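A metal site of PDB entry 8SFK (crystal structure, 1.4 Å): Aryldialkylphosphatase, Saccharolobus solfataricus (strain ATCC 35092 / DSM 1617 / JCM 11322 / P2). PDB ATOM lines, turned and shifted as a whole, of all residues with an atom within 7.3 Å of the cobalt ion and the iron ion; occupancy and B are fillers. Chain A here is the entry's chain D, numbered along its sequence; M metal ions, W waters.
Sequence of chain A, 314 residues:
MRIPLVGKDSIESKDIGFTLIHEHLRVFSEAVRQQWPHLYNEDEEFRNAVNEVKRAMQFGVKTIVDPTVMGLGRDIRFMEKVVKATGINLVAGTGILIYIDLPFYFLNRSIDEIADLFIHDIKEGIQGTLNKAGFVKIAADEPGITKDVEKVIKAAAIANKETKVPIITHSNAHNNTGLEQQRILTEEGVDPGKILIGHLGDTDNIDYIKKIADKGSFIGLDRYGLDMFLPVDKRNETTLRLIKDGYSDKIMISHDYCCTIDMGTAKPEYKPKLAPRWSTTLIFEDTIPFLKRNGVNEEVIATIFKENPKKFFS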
ATOM      1  N   HIS A  22      33.363   2.461   3.400  1.00  0.00           N
ATOM      2  CA  HIS A  22      32.341   3.524   3.379  1.00  0.00           C
ATOM      3  C   HIS A  22      31.574   3.455   2.064  1.00  0.00           C
ATOM      4  O   HIS A  22      31.944   4.120   1.085  1.00  0.00           O
ATOM      5  CB  HIS A  22      32.978   4.889   3.613  1.00  0.00           C
ATOM      6  CG  HIS A  22      31.990   5.984   3.889  1.00  0.00           C
ATOM      7  ND1 HIS A  22      32.183   6.925   4.879  1.00  0.00           N
ATOM      8  CD2 HIS A  22      30.804   6.295   3.309  1.00  0.00           C
ATOM      9  CE1 HIS A  22      31.169   7.761   4.900  1.00  0.00           C
ATOM     10  NE2 HIS A  22      30.319   7.410   3.959  1.00  0.00           N
ATOM     11  N   GLU A  23      30.497   2.667   2.046  1.00  0.00           N
ATOM     12  CA  GLU A  23      29.580   2.575   0.907  1.00  0.00           C
ATOM     13  C   GLU A  23      28.155   2.500   1.431  1.00  0.00           C
ATOM     14  O   GLU A  23      27.938   2.074   2.563  1.00  0.00           O
ATOM     15  CB  GLU A  23      29.863   1.311   0.057  1.00  0.00           C
ATOM     16  CG  GLU A  23      31.359   1.104  -0.273  1.00  0.00           C
ATOM     17  CD  GLU A  23      31.908   2.101  -1.285  1.00  0.00           C
ATOM     18  OE1 GLU A  23      33.147   2.219  -1.384  1.00  0.00           O
ATOM     19  OE2 GLU A  23      31.106   2.757  -1.978  1.00  0.00           O
ATOM     20  N   HIS A  24      27.192   2.928   0.615  1.00  0.00           N
ATOM     21  CA  HIS A  24      25.790   2.968   1.035  1.00  0.00           C
ATOM     22  C   HIS A  24      24.942   2.109   0.119  1.00  0.00           C
ATOM     23  O   HIS A  24      24.862   2.374  -1.089  1.00  0.00           O
ATOM     24  CB  HIS A  24      25.233   4.402   0.980  1.00  0.00           C
ATOM     25  CG  HIS A  24      25.928   5.366   1.906  1.00  0.00           C
ATOM     26  ND1 HIS A  24      25.548   5.532   3.214  1.00  0.00           N
ATOM     27  CD2 HIS A  24      26.960   6.221   1.693  1.00  0.00           C
ATOM     28  CE1 HIS A  24      26.314   6.450   3.770  1.00  0.00           C
ATOM     29  NE2 HIS A  24      27.180   6.903   2.876  1.00  0.00           N
ATOM     30  N   VAL A  27      20.351   5.406   0.300  1.00  0.00           N
ATOM     31  CA  VAL A  27      20.182   6.601   1.126  1.00  0.00           C
ATOM     32  C   VAL A  27      18.858   7.275   0.792  1.00  0.00           C
ATOM     33  O   VAL A  27      18.483   7.398  -0.382  1.00  0.00           O
ATOM     34  CB  VAL A  27      21.347   7.592   0.900  1.00  0.00           C
ATOM     35  CG1 VAL A  27      21.050   8.925   1.555  1.00  0.00           C
ATOM     36  CG2 VAL A  27      22.639   6.989   1.435  1.00  0.00           C
ATOM     37  N   ASP A  66      28.721  -0.078   5.904  1.00  0.00           N
ATOM     38  CA  ASP A  66      27.701   0.821   5.391  1.00  0.00           C
ATOM     39  C   ASP A  66      27.299   1.797   6.487  1.00  0.00           C
ATOM     40  O   ASP A  66      26.571   1.413   7.414  1.00  0.00           O
ATOM     41  CB  ASP A  66      26.491   0.019   4.918  1.00  0.00           C
ATOM     42  CG  ASP A  66      25.381   0.875   4.323  1.00  0.00           C
ATOM     43  OD1 ASP A  66      25.302   2.075   4.665  1.00  0.00           O
ATOM     44  OD2 ASP A  66      24.566   0.373   3.514  1.00  0.00           O
ATOM     45  N   PRO A  67      27.735   3.069   6.429  1.00  0.00           N
ATOM     46  CA  PRO A  67      27.455   4.001   7.526  1.00  0.00           C
ATOM     47  C   PRO A  67      26.171   4.796   7.317  1.00  0.00           C
ATOM     48  O   PRO A  67      26.092   5.963   7.733  1.00  0.00           O
ATOM     49  CB  PRO A  67      28.704   4.892   7.531  1.00  0.00           C
ATOM     50  CG  PRO A  67      29.109   4.957   6.101  1.00  0.00           C
ATOM     51  CD  PRO A  67      28.716   3.606   5.471  1.00  0.00           C
ATOM     52  N   THR A  68      25.161   4.180   6.700  1.00  0.00           N
ATOM     53  CA  THR A  68      23.827   4.765   6.638  1.00  0.00           C
ATOM     54  C   THR A  68      23.205   4.697   8.020  1.00  0.00           C
ATOM     55  O   THR A  68      23.022   3.609   8.577  1.00  0.00           O
ATOM     56  CB  THR A  68      22.955   3.987   5.643  1.00  0.00           C
ATOM     57  OG1 THR A  68      23.625   3.886   4.382  1.00  0.00           O
ATOM     58  CG2 THR A  68      21.624   4.693   5.436  1.00  0.00           C
ATOM     59  N   LEU A  72      20.012   9.424   7.016  1.00  0.00           N
ATOM     60  CA  LEU A  72      20.311   8.843   5.709  1.00  0.00           C
ATOM     61  C   LEU A  72      19.410   7.660   5.367  1.00  0.00           C
ATOM     62  O   LEU A  72      19.593   7.038   4.317  1.00  0.00           O
ATOM     63  CB  LEU A  72      21.781   8.434   5.620  1.00  0.00           C
ATOM     64  CG  LEU A  72      22.818   9.533   5.870  1.00  0.00           C
ATOM     65  CD1 LEU A  72      24.186   8.902   5.880  1.00  0.00           C
ATOM     66  CD2 LEU A  72      22.699  10.602   4.809  1.00  0.00           C
ATOM     67  N   LEU A  97      23.393  11.504  11.592  1.00  0.00           N
ATOM     68  CA  LEU A  97      24.017  12.428  10.643  1.00  0.00           C
ATOM     69  C   LEU A  97      23.167  13.696  10.618  1.00  0.00           C
ATOM     70  O   LEU A  97      22.078  13.712  10.050  1.00  0.00           O
ATOM     71  CB  LEU A  97      24.110  11.800   9.245  1.00  0.00           C
ATOM     72  CG  LEU A  97      24.983  12.696   8.351  1.00  0.00           C
ATOM     73  CD1 LEU A  97      26.058  11.913   7.619  1.00  0.00           C
ATOM     74  CD2 LEU A  97      24.146  13.522   7.393  1.00  0.00           C
ATOM     75  N   TYR A  99      23.826  18.228  10.311  1.00  0.00           N
ATOM     76  CA  TYR A  99      24.745  19.338  10.110  1.00  0.00           C
ATOM     77  C   TYR A  99      24.462  20.527  11.019  1.00  0.00           C
ATOM     78  O   TYR A  99      25.382  21.311  11.267  1.00  0.00           O
ATOM     79  CB  TYR A  99      24.697  19.847   8.667  1.00  0.00           C
ATOM     80  CG  TYR A  99      25.167  18.891   7.578  1.00  0.00           C
ATOM     81  CD1 TYR A  99      25.712  17.648   7.879  1.00  0.00           C
ATOM     82  CD2 TYR A  99      25.070  19.262   6.251  1.00  0.00           C
ATOM     83  CE1 TYR A  99      26.132  16.779   6.857  1.00  0.00           C
ATOM     84  CE2 TYR A  99      25.480  18.421   5.226  1.00  0.00           C
ATOM     85  CZ  TYR A  99      26.009  17.176   5.529  1.00  0.00           C
ATOM     86  OH  TYR A  99      26.422  16.357   4.500  1.00  0.00           O
ATOM     87  N   KCX A 137      28.465   6.305  13.689  1.00  0.00           N
ATOM     88  CA  KCX A 137      28.663   7.303  12.644  1.00  0.00           C
ATOM     89  CB  KCX A 137      27.883   6.889  11.389  1.00  0.00           C
ATOM     90  CG  KCX A 137      27.824   7.921  10.268  1.00  0.00           C
ATOM     91  CD  KCX A 137      29.187   8.192   9.657  1.00  0.00           C
ATOM     92  CE  KCX A 137      29.095   9.209   8.529  1.00  0.00           C
ATOM     93  NZ  KCX A 137      28.328   8.624   7.381  1.00  0.00           N
ATOM     94  C   KCX A 137      28.171   8.663  13.119  1.00  0.00           C
ATOM     95  O   KCX A 137      27.054   8.775  13.644  1.00  0.00           O
ATOM     96  CX  KCX A 137      28.456   9.133   6.160  1.00  0.00           C
ATOM     97  OQ1 KCX A 137      27.794   8.635   5.222  1.00  0.00           O
ATOM     98  OQ2 KCX A 137      29.228  10.115   5.973  1.00  0.00           O
ATOM     99  N   ILE A 138      29.019   9.692  12.951  1.00  0.00           N
ATOM    100  CA  ILE A 138      28.677  11.080  13.301  1.00  0.00           C
ATOM    101  C   ILE A 138      29.086  12.008  12.176  1.00  0.00           C
ATOM    102  O   ILE A 138      29.840  11.606  11.278  1.00  0.00           O
ATOM    103  CB  ILE A 138      29.300  11.522  14.647  1.00  0.00           C
ATOM    104  CG1 ILE A 138      30.831  11.595  14.562  1.00  0.00           C
ATOM    105  CG2 ILE A 138      28.869  10.583  15.771  1.00  0.00           C
ATOM    106  CD1 ILE A 138      31.385  12.983  14.280  1.00  0.00           C
ATOM    107  N   ALA A 139      28.613  13.258  12.209  1.00  0.00           N
ATOM    108  CA  ALA A 139      28.872  14.184  11.113  1.00  0.00           C
ATOM    109  C   ALA A 139      29.105  15.608  11.591  1.00  0.00           C
ATOM    110  O   ALA A 139      28.713  16.005  12.686  1.00  0.00           O
ATOM    111  CB  ALA A 139      27.708  14.231  10.109  1.00  0.00           C
ATOM    112  N   ASP A 141      29.602  19.487   8.984  1.00  0.00           N
ATOM    113  CA  ASP A 141      29.853  19.957   7.636  1.00  0.00           C
ATOM    114  C   ASP A 141      30.081  21.459   7.653  1.00  0.00           C
ATOM    115  O   ASP A 141      30.683  21.977   8.605  1.00  0.00           O
ATOM    116  CB  ASP A 141      28.728  19.529   6.689  1.00  0.00           C
ATOM    117  CG  ASP A 141      29.181  19.400   5.233  1.00  0.00           C
ATOM    118  OD1 ASP A 141      29.354  20.449   4.577  1.00  0.00           O
ATOM    119  OD2 ASP A 141      29.381  18.268   4.745  1.00  0.00           O
ATOM    120  N   THR A 169      33.420   9.089  10.829  1.00  0.00           N
ATOM    121  CA  THR A 169      32.845  10.419  10.686  1.00  0.00           C
ATOM    122  C   THR A 169      32.631  10.814   9.226  1.00  0.00           C
ATOM    123  O   THR A 169      33.264  10.298   8.294  1.00  0.00           O
ATOM    124  CB  THR A 169      33.665  11.541  11.381  1.00  0.00           C
ATOM    125  OG1 THR A 169      34.670  12.044  10.488  1.00  0.00           O
ATOM    126  CG2 THR A 169      34.304  11.064  12.670  1.00  0.00           C
ATOM    127  N   HIS A 170      31.688  11.738   9.071  1.00  0.00           N
ATOM    128  CA  HIS A 170      31.529  12.589   7.912  1.00  0.00           C
ATOM    129  C   HIS A 170      32.065  13.953   8.301  1.00  0.00           C
ATOM    130  O   HIS A 170      31.676  14.492   9.347  1.00  0.00           O
ATOM    131  CB  HIS A 170      30.032  12.711   7.611  1.00  0.00           C
ATOM    132  CG  HIS A 170      29.674  13.734   6.575  1.00  0.00           C
ATOM    133  ND1 HIS A 170      29.180  13.403   5.334  1.00  0.00           N
ATOM    134  CD2 HIS A 170      29.723  15.089   6.614  1.00  0.00           C
ATOM    135  CE1 HIS A 170      28.932  14.513   4.651  1.00  0.00           C
ATOM    136  NE2 HIS A 170      29.257  15.552   5.407  1.00  0.00           N
ATOM    137  N   SER A 171      32.960  14.515   7.502  1.00  0.00           N
ATOM    138  CA  SER A 171      33.427  15.879   7.737  1.00  0.00           C
ATOM    139  C   SER A 171      33.426  16.645   6.413  1.00  0.00           C
ATOM    140  O   SER A 171      33.207  16.073   5.341  1.00  0.00           O
ATOM    141  CB  SER A 171      34.810  15.917   8.421  1.00  0.00           C
ATOM    142  OG  SER A 171      35.890  15.788   7.501  1.00  0.00           O
ATOM    143  N   GLY A 198      36.304  11.215   8.114  1.00  0.00           N
ATOM    144  CA  GLY A 198      35.816  10.998   6.769  1.00  0.00           C
ATOM    145  C   GLY A 198      35.929  12.186   5.838  1.00  0.00           C
ATOM    146  O   GLY A 198      35.984  13.351   6.239  1.00  0.00           O
ATOM    147  N   HIS A 199      35.982  11.852   4.547  1.00  0.00           N
ATOM    148  CA  HIS A 199      35.878  12.781   3.434  1.00  0.00           C
ATOM    149  C   HIS A 199      37.106  13.662   3.258  1.00  0.00           C
ATOM    150  O   HIS A 199      37.055  14.688   2.581  1.00  0.00           O
ATOM    151  CB  HIS A 199      34.566  13.584   3.456  1.00  0.00           C
ATOM    152  CG  HIS A 199      33.346  12.716   3.583  1.00  0.00           C
ATOM    153  ND1 HIS A 199      33.294  11.423   3.103  1.00  0.00           N
ATOM    154  CD2 HIS A 199      32.131  12.959   4.127  1.00  0.00           C
ATOM    155  CE1 HIS A 199      32.110  10.906   3.378  1.00  0.00           C
ATOM    156  NE2 HIS A 199      31.383  11.814   3.992  1.00  0.00           N
ATOM    157  N   ASP A 222      37.760   8.692   0.690  1.00  0.00           N
ATOM    158  CA  ASP A 222      36.599   7.808   0.711  1.00  0.00           C
ATOM    159  C   ASP A 222      35.491   8.197  -0.255  1.00  0.00           C
ATOM    160  O   ASP A 222      34.379   7.674  -0.142  1.00  0.00           O
ATOM    161  CB  ASP A 222      36.075   7.668   2.148  1.00  0.00           C
ATOM    162  CG  ASP A 222      35.684   8.999   2.771  1.00  0.00           C
ATOM    163  OD1 ASP A 222      35.459   9.957   2.020  1.00  0.00           O
ATOM    164  OD2 ASP A 222      35.589   9.066   4.013  1.00  0.00           O
ATOM    165  N   ARG A 223      35.753   9.080  -1.221  1.00  0.00           N
ATOM    166  CA  ARG A 223      34.730   9.544  -2.143  1.00  0.00           C
ATOM    167  C   ARG A 223      35.193   9.430  -3.583  1.00  0.00           C
ATOM    168  O   ARG A 223      34.842  10.254  -4.443  1.00  0.00           O
ATOM    169  CB  ARG A 223      34.256  10.960  -1.811  1.00  0.00           C
ATOM    170  CG  ARG A 223      33.281  10.966  -0.650  1.00  0.00           C
ATOM    171  CD  ARG A 223      32.900  12.395  -0.277  1.00  0.00           C
ATOM    172  NE  ARG A 223      31.559  12.439   0.291  1.00  0.00           N
ATOM    173  CZ  ARG A 223      31.029  13.522   0.851  1.00  0.00           C
ATOM    174  NH1 ARG A 223      31.726  14.648   0.914  1.00  0.00           N
ATOM    175  NH2 ARG A 223      29.798  13.471   1.348  1.00  0.00           N
ATOM    176  N   HIS A 255      34.425   4.695  -1.855  1.00  0.00           N
ATOM    177  CA  HIS A 255      33.758   5.504  -2.860  1.00  0.00           C
ATOM    178  C   HIS A 255      32.608   6.332  -2.324  1.00  0.00           C
ATOM    179  O   HIS A 255      32.183   7.266  -3.027  1.00  0.00           O
ATOM    180  CB  HIS A 255      33.194   4.649  -4.011  1.00  0.00           C
ATOM    181  CG  HIS A 255      34.157   3.638  -4.560  1.00  0.00           C
ATOM    182  ND1 HIS A 255      34.293   2.378  -4.011  1.00  0.00           N
ATOM    183  CD2 HIS A 255      34.973   3.673  -5.634  1.00  0.00           C
ATOM    184  CE1 HIS A 255      35.170   1.688  -4.726  1.00  0.00           C
ATOM    185  NE2 HIS A 255      35.598   2.450  -5.713  1.00  0.00           N
ATOM    186  N   ASP A 256      32.048   5.997  -1.168  1.00  0.00           N
ATOM    187  CA  ASP A 256      30.832   6.651  -0.686  1.00  0.00           C
ATOM    188  C   ASP A 256      29.704   6.460  -1.688  1.00  0.00           C
ATOM    189  O   ASP A 256      28.796   7.301  -1.793  1.00  0.00           O
ATOM    190  CB  ASP A 256      31.074   8.144  -0.412  1.00  0.00           C
ATOM    191  CG  ASP A 256      30.082   8.745   0.573  1.00  0.00           C
ATOM    192  OD1 ASP A 256      29.323   7.992   1.219  1.00  0.00           O
ATOM    193  OD2 ASP A 256      30.096   9.992   0.703  1.00  0.00           O
ATOM    194  N   TYR A 257      29.746   5.372  -2.448  1.00  0.00           N
ATOM    195  CA  TYR A 257      28.773   5.183  -3.499  1.00  0.00           C
ATOM    196  C   TYR A 257      27.421   4.917  -2.881  1.00  0.00           C
ATOM    197  O   TYR A 257      27.302   4.204  -1.879  1.00  0.00           O
ATOM    198  CB  TYR A 257      29.151   4.026  -4.423  1.00  0.00           C
ATOM    199  CG  TYR A 257      28.199   3.924  -5.598  1.00  0.00           C
ATOM    200  CD1 TYR A 257      28.111   4.957  -6.523  1.00  0.00           C
ATOM    201  CD2 TYR A 257      27.380   2.820  -5.759  1.00  0.00           C
ATOM    202  CE1 TYR A 257      27.240   4.887  -7.582  1.00  0.00           C
ATOM    203  CE2 TYR A 257      26.504   2.741  -6.819  1.00  0.00           C
ATOM    204  CZ  TYR A 257      26.434   3.775  -7.730  1.00  0.00           C
ATOM    205  OH  TYR A 257      25.560   3.682  -8.785  1.00  0.00           O
ATOM    206  N   CYS A 258      26.393   5.499  -3.467  1.00  0.00           N
ATOM    207  CA  CYS A 258      25.026   5.267  -3.036  1.00  0.00           C
ATOM    208  C   CYS A 258      24.338   4.520  -4.157  1.00  0.00           C
ATOM    209  O   CYS A 258      24.121   5.072  -5.240  1.00  0.00           O
ATOM    210  CB  CYS A 258      24.319   6.585  -2.737  1.00  0.00           C
ATOM    211  SG  CYS A 258      25.114   7.533  -1.424  1.00  0.00           S
HETATM  212 CO    CO M   1      29.340  11.499   4.450  1.00  0.00          CO
HETATM  213 FE    FE M   2      28.558   8.416   3.270  1.00  0.00          FE
HETATM  214  O   HOH W   1      28.897  10.316   3.031  1.00  0.00           O
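NE2 of His 170 lies within hydrogen-bond range of OD2 of Asp 141. OH of Tyr 99 sits at hydrogen-bond distance from NE2 of His 170, at 3.1 Å. ND1 of His 199 is in hydrogen-bond range of NE of Arg 223 (3.5 Å). The backbone carbonyl oxygen (O) of Ile 138 is in hydrogen-bond range of the backbone NH (N) of His 170. The backbone carbonyl oxygen of Tyr 257 is in hydrogen-bond range of the backbone NH of His 24, at 2.8 Å. The guanidinium group (NE) of Arg 223 is in salt-bridge range of the side-chain carboxylate (OD2) of Asp 256. The side-chain hydroxyl of Thr 68 is in hydrogen-bond range of a ring nitrogen (ND1) of His 24 (2.8 Å). NZ of KCX 137 sits at hydrogen-bond distance from O of Pro 67 (3.5 Å).
Arg 223 touches the cobalt ion. Four residues have an atom within 4 Å of the cobalt ion: KCX 137, His 170, His 199 and Arg 223. The nearest printed residue that does not touch the cobalt ion is Asp 256 (4.1 Å).
Of the 25 residues printed, 4 come within 4 Å of the iron ion.
Water W1 is bound to the cobalt ion, 1.9 Å away. OQ2 of KCX 137 is bound to the cobalt ion. The cobalt ion is bound by ND1 of His 170. The cobalt ion is bound by NE2 of His 199, at 2.1 Å. The cobalt ion has four donor atoms within binding distance.
The iron ion is bound by water W1, NE2 of His 24, OQ1 of KCX 137, NE2 of His 22 and OD1 of Asp 256.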
